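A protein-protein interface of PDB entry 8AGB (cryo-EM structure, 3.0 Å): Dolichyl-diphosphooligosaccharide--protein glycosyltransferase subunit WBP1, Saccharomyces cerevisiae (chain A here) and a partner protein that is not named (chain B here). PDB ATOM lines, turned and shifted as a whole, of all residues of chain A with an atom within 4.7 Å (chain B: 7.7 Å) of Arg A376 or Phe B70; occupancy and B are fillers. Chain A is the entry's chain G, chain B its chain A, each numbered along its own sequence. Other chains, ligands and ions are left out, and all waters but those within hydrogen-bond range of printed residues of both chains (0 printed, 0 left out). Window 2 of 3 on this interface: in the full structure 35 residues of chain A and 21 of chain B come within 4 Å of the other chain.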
ATOM      1  N   PRO A 283       6.137  -4.389  11.794  1.00  0.00           N
ATOM      2  CA  PRO A 283       7.276  -4.692  12.673  1.00  0.00           C
ATOM      3  C   PRO A 283       8.337  -3.602  12.692  1.00  0.00           C
ATOM      4  O   PRO A 283       8.460  -2.821  11.745  1.00  0.00           O
ATOM      5  CB  PRO A 283       7.825  -5.996  12.088  1.00  0.00           C
ATOM      6  CG  PRO A 283       6.647  -6.637  11.461  1.00  0.00           C
ATOM      7  CD  PRO A 283       5.803  -5.520  10.915  1.00  0.00           C
ATOM      8  N   TYR A 284       9.116  -3.553  13.767  1.00  0.00           N
ATOM      9  CA  TYR A 284      10.096  -2.500  13.954  1.00  0.00           C
ATOM     10  C   TYR A 284      11.327  -2.735  13.087  1.00  0.00           C
ATOM     11  O   TYR A 284      11.607  -3.848  12.641  1.00  0.00           O
ATOM     12  CB  TYR A 284      10.514  -2.413  15.419  1.00  0.00           C
ATOM     13  CG  TYR A 284       9.433  -1.908  16.335  1.00  0.00           C
ATOM     14  CD1 TYR A 284       8.447  -1.053  15.871  1.00  0.00           C
ATOM     15  CD2 TYR A 284       9.396  -2.286  17.667  1.00  0.00           C
ATOM     16  CE1 TYR A 284       7.458  -0.590  16.706  1.00  0.00           C
ATOM     17  CE2 TYR A 284       8.410  -1.830  18.507  1.00  0.00           C
ATOM     18  CZ  TYR A 284       7.445  -0.983  18.023  1.00  0.00           C
ATOM     19  OH  TYR A 284       6.463  -0.526  18.862  1.00  0.00           O
ATOM     20  N   LYS A 285      12.067  -1.654  12.853  1.00  0.00           N
ATOM     21  CA  LYS A 285      13.346  -1.699  12.162  1.00  0.00           C
ATOM     22  C   LYS A 285      14.274  -0.690  12.822  1.00  0.00           C
ATOM     23  O   LYS A 285      13.882   0.032  13.743  1.00  0.00           O
ATOM     24  CB  LYS A 285      13.177  -1.414  10.668  1.00  0.00           C
ATOM     25  CG  LYS A 285      12.571  -0.060  10.385  1.00  0.00           C
ATOM     26  CD  LYS A 285      12.486   0.224   8.902  1.00  0.00           C
ATOM     27  CE  LYS A 285      12.227   1.697   8.658  1.00  0.00           C
ATOM     28  NZ  LYS A 285      11.644   1.950   7.315  1.00  0.00           N
ATOM     29  N   ILE A 286      15.519  -0.637  12.350  1.00  0.00           N
ATOM     30  CA  ILE A 286      16.496   0.261  12.950  1.00  0.00           C
ATOM     31  C   ILE A 286      16.153   1.703  12.603  1.00  0.00           C
ATOM     32  O   ILE A 286      15.716   2.009  11.485  1.00  0.00           O
ATOM     33  CB  ILE A 286      17.920  -0.111  12.499  1.00  0.00           C
ATOM     34  CG1 ILE A 286      18.105   0.147  11.004  1.00  0.00           C
ATOM     35  CG2 ILE A 286      18.223  -1.557  12.838  1.00  0.00           C
ATOM     36  CD1 ILE A 286      19.344  -0.491  10.425  1.00  0.00           C
ATOM     37  N   HIS A 350      20.527  -3.967  14.744  1.00  0.00           N
ATOM     38  CA  HIS A 350      19.411  -4.898  14.725  1.00  0.00           C
ATOM     39  C   HIS A 350      19.596  -5.975  15.787  1.00  0.00           C
ATOM     40  O   HIS A 350      20.693  -6.184  16.310  1.00  0.00           O
ATOM     41  CB  HIS A 350      19.279  -5.546  13.350  1.00  0.00           C
ATOM     42  CG  HIS A 350      20.461  -6.375  12.962  1.00  0.00           C
ATOM     43  ND1 HIS A 350      21.493  -5.888  12.190  1.00  0.00           N
ATOM     44  CD2 HIS A 350      20.773  -7.663  13.236  1.00  0.00           C
ATOM     45  CE1 HIS A 350      22.391  -6.838  12.007  1.00  0.00           C
ATOM     46  NE2 HIS A 350      21.978  -7.926  12.632  1.00  0.00           N
ATOM     47  N   GLY A 351      18.513  -6.659  16.107  1.00  0.00           N
ATOM     48  CA  GLY A 351      18.599  -7.756  17.052  1.00  0.00           C
ATOM     49  C   GLY A 351      17.356  -7.841  17.909  1.00  0.00           C
ATOM     50  O   GLY A 351      16.446  -7.028  17.813  1.00  0.00           O
ATOM     51  N   ALA A 374      11.839  -7.908  18.170  1.00  0.00           N
ATOM     52  CA  ALA A 374      12.940  -8.088  17.230  1.00  0.00           C
ATOM     53  C   ALA A 374      13.023  -6.871  16.319  1.00  0.00           C
ATOM     54  O   ALA A 374      12.138  -6.653  15.487  1.00  0.00           O
ATOM     55  CB  ALA A 374      12.757  -9.365  16.414  1.00  0.00           C
ATOM     56  N   ILE A 375      14.082  -6.082  16.474  1.00  0.00           N
ATOM     57  CA  ILE A 375      14.317  -4.918  15.629  1.00  0.00           C
ATOM     58  C   ILE A 375      15.044  -5.401  14.381  1.00  0.00           C
ATOM     59  O   ILE A 375      16.189  -5.862  14.451  1.00  0.00           O
ATOM     60  CB  ILE A 375      15.115  -3.839  16.367  1.00  0.00           C
ATOM     61  CG1 ILE A 375      14.708  -3.800  17.839  1.00  0.00           C
ATOM     62  CG2 ILE A 375      14.897  -2.490  15.727  1.00  0.00           C
ATOM     63  CD1 ILE A 375      13.372  -3.156  18.086  1.00  0.00           C
ATOM     64  N   ARG A 376      14.369  -5.288  13.242  1.00  0.00           N
ATOM     65  CA  ARG A 376      14.808  -5.804  11.957  1.00  0.00           C
ATOM     66  C   ARG A 376      15.857  -4.872  11.349  1.00  0.00           C
ATOM     67  O   ARG A 376      16.238  -3.857  11.934  1.00  0.00           O
ATOM     68  CB  ARG A 376      13.582  -5.974  11.058  1.00  0.00           C
ATOM     69  CG  ARG A 376      13.753  -6.779   9.788  1.00  0.00           C
ATOM     70  CD  ARG A 376      13.092  -6.066   8.620  1.00  0.00           C
ATOM     71  NE  ARG A 376      11.713  -5.687   8.905  1.00  0.00           N
ATOM     72  CZ  ARG A 376      11.135  -4.584   8.443  1.00  0.00           C
ATOM     73  NH1 ARG A 376      11.818  -3.747   7.676  1.00  0.00           N
ATOM     74  NH2 ARG A 376       9.876  -4.314   8.747  1.00  0.00           N
ATOM     75  N   HIS A 377      16.330  -5.212  10.155  1.00  0.00           N
ATOM     76  CA  HIS A 377      17.241  -4.380   9.386  1.00  0.00           C
ATOM     77  C   HIS A 377      16.504  -3.768   8.202  1.00  0.00           C
ATOM     78  O   HIS A 377      15.413  -4.205   7.831  1.00  0.00           O
ATOM     79  CB  HIS A 377      18.446  -5.186   8.890  1.00  0.00           C
ATOM     80  CG  HIS A 377      19.716  -4.396   8.824  1.00  0.00           C
ATOM     81  ND1 HIS A 377      20.699  -4.482   9.786  1.00  0.00           N
ATOM     82  CD2 HIS A 377      20.166  -3.507   7.907  1.00  0.00           C
ATOM     83  CE1 HIS A 377      21.698  -3.681   9.468  1.00  0.00           C
ATOM     84  NE2 HIS A 377      21.400  -3.076   8.332  1.00  0.00           N
ATOM     85  N   LEU A 378      17.106  -2.740   7.614  1.00  0.00           N
ATOM     86  CA  LEU A 378      16.490  -2.090   6.465  1.00  0.00           C
ATOM     87  C   LEU A 378      16.375  -3.064   5.300  1.00  0.00           C
ATOM     88  O   LEU A 378      17.360  -3.688   4.892  1.00  0.00           O
ATOM     89  CB  LEU A 378      17.303  -0.866   6.051  1.00  0.00           C
ATOM     90  CG  LEU A 378      17.168   0.370   6.935  1.00  0.00           C
ATOM     91  CD1 LEU A 378      17.859   1.553   6.288  1.00  0.00           C
ATOM     92  CD2 LEU A 378      15.708   0.680   7.190  1.00  0.00           C
ATOM     93  N   ALA A 379      15.165  -3.193   4.765  1.00  0.00           N
ATOM     94  CA  ALA A 379      14.936  -4.068   3.629  1.00  0.00           C
ATOM     95  C   ALA A 379      15.488  -3.438   2.357  1.00  0.00           C
ATOM     96  O   ALA A 379      15.697  -2.226   2.273  1.00  0.00           O
ATOM     97  CB  ALA A 379      13.444  -4.358   3.467  1.00  0.00           C
ATOM     98  N   GLU A 382      13.657  -0.312   1.353  1.00  0.00           N
ATOM     99  CA  GLU A 382      13.675   0.914   2.150  1.00  0.00           C
ATOM    100  C   GLU A 382      15.072   1.519   2.091  1.00  0.00           C
ATOM    101  O   GLU A 382      15.906   1.344   2.982  1.00  0.00           O
ATOM    102  CB  GLU A 382      13.245   0.626   3.582  1.00  0.00           C
ATOM    103  CG  GLU A 382      11.817   0.138   3.709  1.00  0.00           C
ATOM    104  CD  GLU A 382      11.662  -0.913   4.784  1.00  0.00           C
ATOM    105  OE1 GLU A 382      12.667  -1.231   5.453  1.00  0.00           O
ATOM    106  OE2 GLU A 382      10.537  -1.425   4.960  1.00  0.00           O
ATOM    107  N   ARG B  53      14.859 -25.284   6.482  1.00  0.00           N
ATOM    108  CA  ARG B  53      14.161 -24.219   7.193  1.00  0.00           C
ATOM    109  C   ARG B  53      13.948 -23.007   6.292  1.00  0.00           C
ATOM    110  O   ARG B  53      12.843 -22.452   6.221  1.00  0.00           O
ATOM    111  CB  ARG B  53      14.947 -23.835   8.447  1.00  0.00           C
ATOM    112  CG  ARG B  53      14.183 -22.969   9.425  1.00  0.00           C
ATOM    113  CD  ARG B  53      14.726 -23.131  10.836  1.00  0.00           C
ATOM    114  NE  ARG B  53      15.592 -22.026  11.232  1.00  0.00           N
ATOM    115  CZ  ARG B  53      15.150 -20.844  11.646  1.00  0.00           C
ATOM    116  NH1 ARG B  53      13.848 -20.609  11.718  1.00  0.00           N
ATOM    117  NH2 ARG B  53      16.009 -19.896  11.986  1.00  0.00           N
ATOM    118  N   TYR B  57      10.410 -21.503   4.853  1.00  0.00           N
ATOM    119  CA  TYR B  57      10.021 -20.114   5.076  1.00  0.00           C
ATOM    120  C   TYR B  57       9.659 -19.434   3.761  1.00  0.00           C
ATOM    121  O   TYR B  57       8.614 -18.782   3.654  1.00  0.00           O
ATOM    122  CB  TYR B  57      11.142 -19.356   5.785  1.00  0.00           C
ATOM    123  CG  TYR B  57      10.790 -17.926   6.130  1.00  0.00           C
ATOM    124  CD1 TYR B  57      10.978 -16.899   5.215  1.00  0.00           C
ATOM    125  CD2 TYR B  57      10.265 -17.605   7.372  1.00  0.00           C
ATOM    126  CE1 TYR B  57      10.655 -15.597   5.528  1.00  0.00           C
ATOM    127  CE2 TYR B  57       9.939 -16.304   7.694  1.00  0.00           C
ATOM    128  CZ  TYR B  57      10.137 -15.305   6.769  1.00  0.00           C
ATOM    129  OH  TYR B  57       9.813 -14.007   7.090  1.00  0.00           O
ATOM    130  N   TYR B  64       9.449 -11.978  -1.538  1.00  0.00           N
ATOM    131  CA  TYR B  64       9.948 -10.712  -1.015  1.00  0.00           C
ATOM    132  C   TYR B  64      10.342 -10.846   0.449  1.00  0.00           C
ATOM    133  O   TYR B  64      11.418 -10.396   0.856  1.00  0.00           O
ATOM    134  CB  TYR B  64       8.891  -9.624  -1.194  1.00  0.00           C
ATOM    135  CG  TYR B  64       9.256  -8.293  -0.581  1.00  0.00           C
ATOM    136  CD1 TYR B  64      10.057  -7.391  -1.264  1.00  0.00           C
ATOM    137  CD2 TYR B  64       8.788  -7.935   0.675  1.00  0.00           C
ATOM    138  CE1 TYR B  64      10.389  -6.172  -0.711  1.00  0.00           C
ATOM    139  CE2 TYR B  64       9.115  -6.719   1.237  1.00  0.00           C
ATOM    140  CZ  TYR B  64       9.914  -5.841   0.540  1.00  0.00           C
ATOM    141  OH  TYR B  64      10.244  -4.629   1.096  1.00  0.00           O
ATOM    142  N   LYS B  65       9.479 -11.460   1.258  1.00  0.00           N
ATOM    143  CA  LYS B  65       9.784 -11.652   2.669  1.00  0.00           C
ATOM    144  C   LYS B  65      10.966 -12.584   2.884  1.00  0.00           C
ATOM    145  O   LYS B  65      11.557 -12.573   3.967  1.00  0.00           O
ATOM    146  CB  LYS B  65       8.557 -12.193   3.399  1.00  0.00           C
ATOM    147  CG  LYS B  65       7.466 -11.164   3.606  1.00  0.00           C
ATOM    148  CD  LYS B  65       6.286 -11.759   4.346  1.00  0.00           C
ATOM    149  CE  LYS B  65       6.446 -11.597   5.846  1.00  0.00           C
ATOM    150  NZ  LYS B  65       5.148 -11.294   6.504  1.00  0.00           N
ATOM    151  N   PHE B  66      11.324 -13.387   1.881  1.00  0.00           N
ATOM    152  CA  PHE B  66      12.444 -14.309   2.029  1.00  0.00           C
ATOM    153  C   PHE B  66      13.779 -13.597   1.865  1.00  0.00           C
ATOM    154  O   PHE B  66      14.718 -13.853   2.624  1.00  0.00           O
ATOM    155  CB  PHE B  66      12.316 -15.450   1.020  1.00  0.00           C
ATOM    156  CG  PHE B  66      13.564 -16.268   0.869  1.00  0.00           C
ATOM    157  CD1 PHE B  66      13.973 -17.126   1.873  1.00  0.00           C
ATOM    158  CD2 PHE B  66      14.326 -16.187  -0.284  1.00  0.00           C
ATOM    159  CE1 PHE B  66      15.117 -17.880   1.734  1.00  0.00           C
ATOM    160  CE2 PHE B  66      15.470 -16.939  -0.428  1.00  0.00           C
ATOM    161  CZ  PHE B  66      15.867 -17.786   0.582  1.00  0.00           C
ATOM    162  N   LEU B  67      13.885 -12.706   0.878  1.00  0.00           N
ATOM    163  CA  LEU B  67      15.143 -12.001   0.660  1.00  0.00           C
ATOM    164  C   LEU B  67      15.418 -10.993   1.765  1.00  0.00           C
ATOM    165  O   LEU B  67      16.580 -10.673   2.035  1.00  0.00           O
ATOM    166  CB  LEU B  67      15.126 -11.308  -0.699  1.00  0.00           C
ATOM    167  CG  LEU B  67      15.057 -12.223  -1.922  1.00  0.00           C
ATOM    168  CD1 LEU B  67      14.821 -11.405  -3.175  1.00  0.00           C
ATOM    169  CD2 LEU B  67      16.325 -13.043  -2.045  1.00  0.00           C
ATOM    170  N   ASN B  68      14.370 -10.482   2.411  1.00  0.00           N
ATOM    171  CA  ASN B  68      14.502  -9.587   3.551  1.00  0.00           C
ATOM    172  C   ASN B  68      14.177 -10.294   4.862  1.00  0.00           C
ATOM    173  O   ASN B  68      13.616  -9.693   5.780  1.00  0.00           O
ATOM    174  CB  ASN B  68      13.614  -8.360   3.372  1.00  0.00           C
ATOM    175  CG  ASN B  68      13.500  -7.939   1.929  1.00  0.00           C
ATOM    176  OD1 ASN B  68      14.469  -7.996   1.177  1.00  0.00           O
ATOM    177  ND2 ASN B  68      12.311  -7.518   1.530  1.00  0.00           N
ATOM    178  N   TRP B  69      14.515 -11.574   4.953  1.00  0.00           N
ATOM    179  CA  TRP B  69      14.245 -12.346   6.154  1.00  0.00           C
ATOM    180  C   TRP B  69      15.199 -11.933   7.264  1.00  0.00           C
ATOM    181  O   TRP B  69      16.348 -11.572   7.015  1.00  0.00           O
ATOM    182  CB  TRP B  69      14.392 -13.838   5.864  1.00  0.00           C
ATOM    183  CG  TRP B  69      13.972 -14.744   6.977  1.00  0.00           C
ATOM    184  CD1 TRP B  69      13.138 -14.446   8.012  1.00  0.00           C
ATOM    185  CD2 TRP B  69      14.373 -16.104   7.165  1.00  0.00           C
ATOM    186  NE1 TRP B  69      12.996 -15.535   8.834  1.00  0.00           N
ATOM    187  CE2 TRP B  69      13.745 -16.567   8.333  1.00  0.00           C
ATOM    188  CE3 TRP B  69      15.201 -16.976   6.455  1.00  0.00           C
ATOM    189  CZ2 TRP B  69      13.917 -17.861   8.808  1.00  0.00           C
ATOM    190  CZ3 TRP B  69      15.372 -18.258   6.930  1.00  0.00           C
ATOM    191  CH2 TRP B  69      14.734 -18.689   8.094  1.00  0.00           C
ATOM    192  N   PHE B  70      14.703 -11.956   8.499  1.00  0.00           N
ATOM    193  CA  PHE B  70      15.551 -11.731   9.667  1.00  0.00           C
ATOM    194  C   PHE B  70      14.993 -12.612  10.778  1.00  0.00           C
ATOM    195  O   PHE B  70      13.956 -12.290  11.365  1.00  0.00           O
ATOM    196  CB  PHE B  70      15.581 -10.260  10.067  1.00  0.00           C
ATOM    197  CG  PHE B  70      16.097 -10.018  11.460  1.00  0.00           C
ATOM    198  CD1 PHE B  70      17.455  -9.921  11.697  1.00  0.00           C
ATOM    199  CD2 PHE B  70      15.229  -9.862  12.524  1.00  0.00           C
ATOM    200  CE1 PHE B  70      17.937  -9.697  12.966  1.00  0.00           C
ATOM    201  CE2 PHE B  70      15.709  -9.639  13.795  1.00  0.00           C
ATOM    202  CZ  PHE B  70      17.064  -9.555  14.016  1.00  0.00           C
ATOM    203  N   ASP B  71      15.658 -13.733  11.037  1.00  0.00           N
ATOM    204  CA  ASP B  71      15.171 -14.695  12.015  1.00  0.00           C
ATOM    205  C   ASP B  71      15.766 -14.413  13.388  1.00  0.00           C
ATOM    206  O   ASP B  71      16.965 -14.154  13.517  1.00  0.00           O
ATOM    207  CB  ASP B  71      15.484 -16.127  11.575  1.00  0.00           C
ATOM    208  CG  ASP B  71      16.963 -16.428  11.568  1.00  0.00           C
ATOM    209  OD1 ASP B  71      17.757 -15.497  11.331  1.00  0.00           O
ATOM    210  OD2 ASP B  71      17.332 -17.597  11.802  1.00  0.00           O
ATOM    211  N   ASP B  72      14.910 -14.437  14.404  1.00  0.00           N
ATOM    212  CA  ASP B  72      15.321 -14.247  15.786  1.00  0.00           C
ATOM    213  C   ASP B  72      15.525 -15.559  16.527  1.00  0.00           C
ATOM    214  O   ASP B  72      15.848 -15.538  17.718  1.00  0.00           O
ATOM    215  CB  ASP B  72      14.291 -13.391  16.525  1.00  0.00           C
ATOM    216  CG  ASP B  72      12.870 -13.711  16.116  1.00  0.00           C
ATOM    217  OD1 ASP B  72      12.682 -14.292  15.028  1.00  0.00           O
ATOM    218  OD2 ASP B  72      11.939 -13.385  16.883  1.00  0.00           O
ATOM    219  N   ARG B  73      15.349 -16.697  15.856  1.00  0.00           N
ATOM    220  CA  ARG B  73      15.501 -18.002  16.482  1.00  0.00           C
ATOM    221  C   ARG B  73      16.908 -18.566  16.343  1.00  0.00           C
ATOM    222  O   ARG B  73      17.096 -19.776  16.503  1.00  0.00           O
ATOM    223  CB  ARG B  73      14.491 -18.989  15.895  1.00  0.00           C
ATOM    224  CG  ARG B  73      13.236 -18.346  15.345  1.00  0.00           C
ATOM    225  CD  ARG B  73      12.140 -18.334  16.387  1.00  0.00           C
ATOM    226  NE  ARG B  73      11.584 -19.663  16.609  1.00  0.00           N
ATOM    227  CZ  ARG B  73      10.804 -19.977  17.637  1.00  0.00           C
ATOM    228  NH1 ARG B  73      10.491 -19.057  18.534  1.00  0.00           N
ATOM    229  NH2 ARG B  73      10.340 -21.211  17.770  1.00  0.00           N
ATOM    230  N   THR B  74      17.896 -17.724  16.058  1.00  0.00           N
ATOM    231  CA  THR B  74      19.276 -18.168  15.943  1.00  0.00           C
ATOM    232  C   THR B  74      20.177 -17.064  16.468  1.00  0.00           C
ATOM    233  O   THR B  74      19.889 -15.879  16.279  1.00  0.00           O
ATOM    234  CB  THR B  74      19.644 -18.505  14.494  1.00  0.00           C
ATOM    235  OG1 THR B  74      19.007 -17.573  13.613  1.00  0.00           O
ATOM    236  CG2 THR B  74      19.191 -19.909  14.135  1.00  0.00           C
ATOM    237  N   TYR B  76      20.720 -15.987  19.560  1.00  0.00           N
ATOM    238  CA  TYR B  76      19.549 -15.327  20.130  1.00  0.00           C
ATOM    239  C   TYR B  76      19.730 -13.817  20.275  1.00  0.00           C
ATOM    240  O   TYR B  76      19.018 -13.072  19.592  1.00  0.00           O
ATOM    241  CB  TYR B  76      19.172 -15.961  21.473  1.00  0.00           C
ATOM    242  CG  TYR B  76      18.387 -15.041  22.379  1.00  0.00           C
ATOM    243  CD1 TYR B  76      17.178 -14.491  21.971  1.00  0.00           C
ATOM    244  CD2 TYR B  76      18.863 -14.710  23.638  1.00  0.00           C
ATOM    245  CE1 TYR B  76      16.469 -13.645  22.792  1.00  0.00           C
ATOM    246  CE2 TYR B  76      18.158 -13.866  24.465  1.00  0.00           C
ATOM    247  CZ  TYR B  76      16.963 -13.338  24.038  1.00  0.00           C
ATOM    248  OH  TYR B  76      16.257 -12.494  24.862  1.00  0.00           O
ATOM    249  N   PRO B  77      20.627 -13.307  21.131  1.00  0.00           N
ATOM    250  CA  PRO B  77      20.632 -11.847  21.332  1.00  0.00           C
ATOM    251  C   PRO B  77      20.930 -11.108  20.041  1.00  0.00           C
ATOM    252  O   PRO B  77      20.206 -10.179  19.664  1.00  0.00           O
ATOM    253  CB  PRO B  77      21.722 -11.631  22.393  1.00  0.00           C
ATOM    254  CG  PRO B  77      22.133 -12.976  22.858  1.00  0.00           C
ATOM    255  CD  PRO B  77      21.769 -13.952  21.798  1.00  0.00           C
ATOM    256  N   LEU B  78      21.990 -11.521  19.347  1.00  0.00           N
ATOM    257  CA  LEU B  78      22.482 -10.788  18.188  1.00  0.00           C
ATOM    258  C   LEU B  78      21.546 -10.916  16.993  1.00  0.00           C
ATOM    259  O   LEU B  78      21.248  -9.925  16.318  1.00  0.00           O
ATOM    260  CB  LEU B  78      23.878 -11.286  17.826  1.00  0.00           C
ATOM    261  CG  LEU B  78      24.790 -11.514  19.026  1.00  0.00           C
ATOM    262  CD1 LEU B  78      26.033 -12.254  18.595  1.00  0.00           C
ATOM    263  CD2 LEU B  78      25.146 -10.188  19.666  1.00  0.00           C
ATOM    264  N   GLY B  79      21.077 -12.124  16.712  1.00  0.00           N
ATOM    265  CA  GLY B  79      20.249 -12.350  15.549  1.00  0.00           C
ATOM    266  C   GLY B  79      21.088 -12.586  14.306  1.00  0.00           C
ATOM    267  O   GLY B  79      22.285 -12.311  14.264  1.00  0.00           O
ATOM    268  N   ARG B  80      20.439 -13.105  13.266  1.00  0.00           N
ATOM    269  CA  ARG B  80      21.086 -13.285  11.974  1.00  0.00           C
ATOM    270  C   ARG B  80      20.266 -12.593  10.897  1.00  0.00           C
ATOM    271  O   ARG B  80      19.060 -12.828  10.785  1.00  0.00           O
ATOM    272  CB  ARG B  80      21.241 -14.772  11.653  1.00  0.00           C
ATOM    273  CG  ARG B  80      22.082 -15.069  10.436  1.00  0.00           C
ATOM    274  CD  ARG B  80      22.136 -16.559  10.183  1.00  0.00           C
ATOM    275  NE  ARG B  80      22.564 -16.874   8.827  1.00  0.00           N
ATOM    276  CZ  ARG B  80      22.790 -18.106   8.388  1.00  0.00           C
ATOM    277  NH1 ARG B  80      22.638 -19.137   9.206  1.00  0.00           N
ATOM    278  NH2 ARG B  80      23.178 -18.309   7.138  1.00  0.00           N
ATOM    279  N   VAL B  81      20.927 -11.748  10.103  1.00  0.00           N
ATOM    280  CA  VAL B  81      20.229 -11.032   9.041  1.00  0.00           C
ATOM    281  C   VAL B  81      19.819 -11.963   7.906  1.00  0.00           C
ATOM    282  O   VAL B  81      18.881 -11.656   7.166  1.00  0.00           O
ATOM    283  CB  VAL B  81      21.091  -9.858   8.536  1.00  0.00           C
ATOM    284  CG1 VAL B  81      22.197 -10.348   7.619  1.00  0.00           C
ATOM    285  CG2 VAL B  81      20.226  -8.830   7.833  1.00  0.00           C
ATOM    286  N   THR B  82      20.555 -13.053   7.685  1.00  0.00           N
ATOM    287  CA  THR B  82      20.215 -14.073   6.692  1.00  0.00           C
ATOM    288  C   THR B  82      20.320 -13.558   5.259  1.00  0.00           C
ATOM    289  O   THR B  82      20.826 -14.263   4.381  1.00  0.00           O
ATOM    290  CB  THR B  82      18.811 -14.638   6.938  1.00  0.00           C
ATOM    291  OG1 THR B  82      18.731 -15.170   8.265  1.00  0.00           O
ATOM    292  CG2 THR B  82      18.504 -15.744   5.948  1.00  0.00           C
ATOM    293  N   GLY B  83      19.845 -12.335   5.012  1.00  0.00           N
ATOM    294  CA  GLY B  83      19.832 -11.813   3.653  1.00  0.00           C
ATOM    295  C   GLY B  83      21.217 -11.713   3.048  1.00  0.00           C
ATOM    296  O   GLY B  83      21.414 -12.005   1.867  1.00  0.00           O
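O of Tyr B64 lies within hydrogen-bond range of ND2 of Asn B68 (3.1 Å).
A ring nitrogen (ND1) of His A350 sits at hydrogen-bond distance from a ring nitrogen (ND1) of His A377.
The backbone NH of Ala A379 sits at hydrogen-bond distance from the side-chain carboxylate of Glu A382 (3.3 Å).
N of Ile A286 sits close to O of Arg A376 (3.3 Å).
NH1 of Arg A376 lies within salt-bridge range of OE1 of Glu A382, at 3.5 Å.
The backbone NH of Arg A376 lies within hydrogen-bond range of the backbone carbonyl oxygen of Tyr A284.
His A350 touches Phe B70 (CD2 to CE1, 3.5 Å).
O of Leu B78 touches O of His A350 (3.8 Å).
CA of Gly A351 touches CZ of Phe B70, 3.8 Å away.
CA of Gly A351 touches O of Pro B77 (3.9 Å).
Gly A351 touches Leu B78.
CB of Ala A374 touches CE2 of Phe B70, 3.96 Å away.
Ile A375 touches Phe B70.
Arg A376 touches Phe B70.
OH of Tyr B64 touches CB of Ala A379, at 3.99 Å.
Ala A379 touches Asn B68 (CB to ND2, 3.9 Å).
Of chain B, only Phe B70 (3.9 Å) comes within 4 Å of Arg A376.
Phe B70 touches five residues of chain A.
Of the printed residues of chain B, Ala A374 touches Phe B70.
Of the printed residues of chain B, His A350 touches Phe B70 and Leu B78.
The nearest printed residue of chain A that does not touch Phe B70 is His A377 (5.0 Å).
The nearest printed residue of chain B that does not touch Ile A375 is Leu B78 (6.8 Å).
Printed residues of chain A that touch a printed residue of chain B: His A350, Gly A351, Ala A374, Ile A375, Arg A376 and Ala A379.
Of the 21 printed residues of chain B, 5 touch a printed residue of chain A.
Among the printed residues, 10 pairs touch across the chains.
Among the printed residues, no Asp or Glu carboxylate lies within 4 Å of a Lys or Arg side-chain nitrogen of the other chain.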
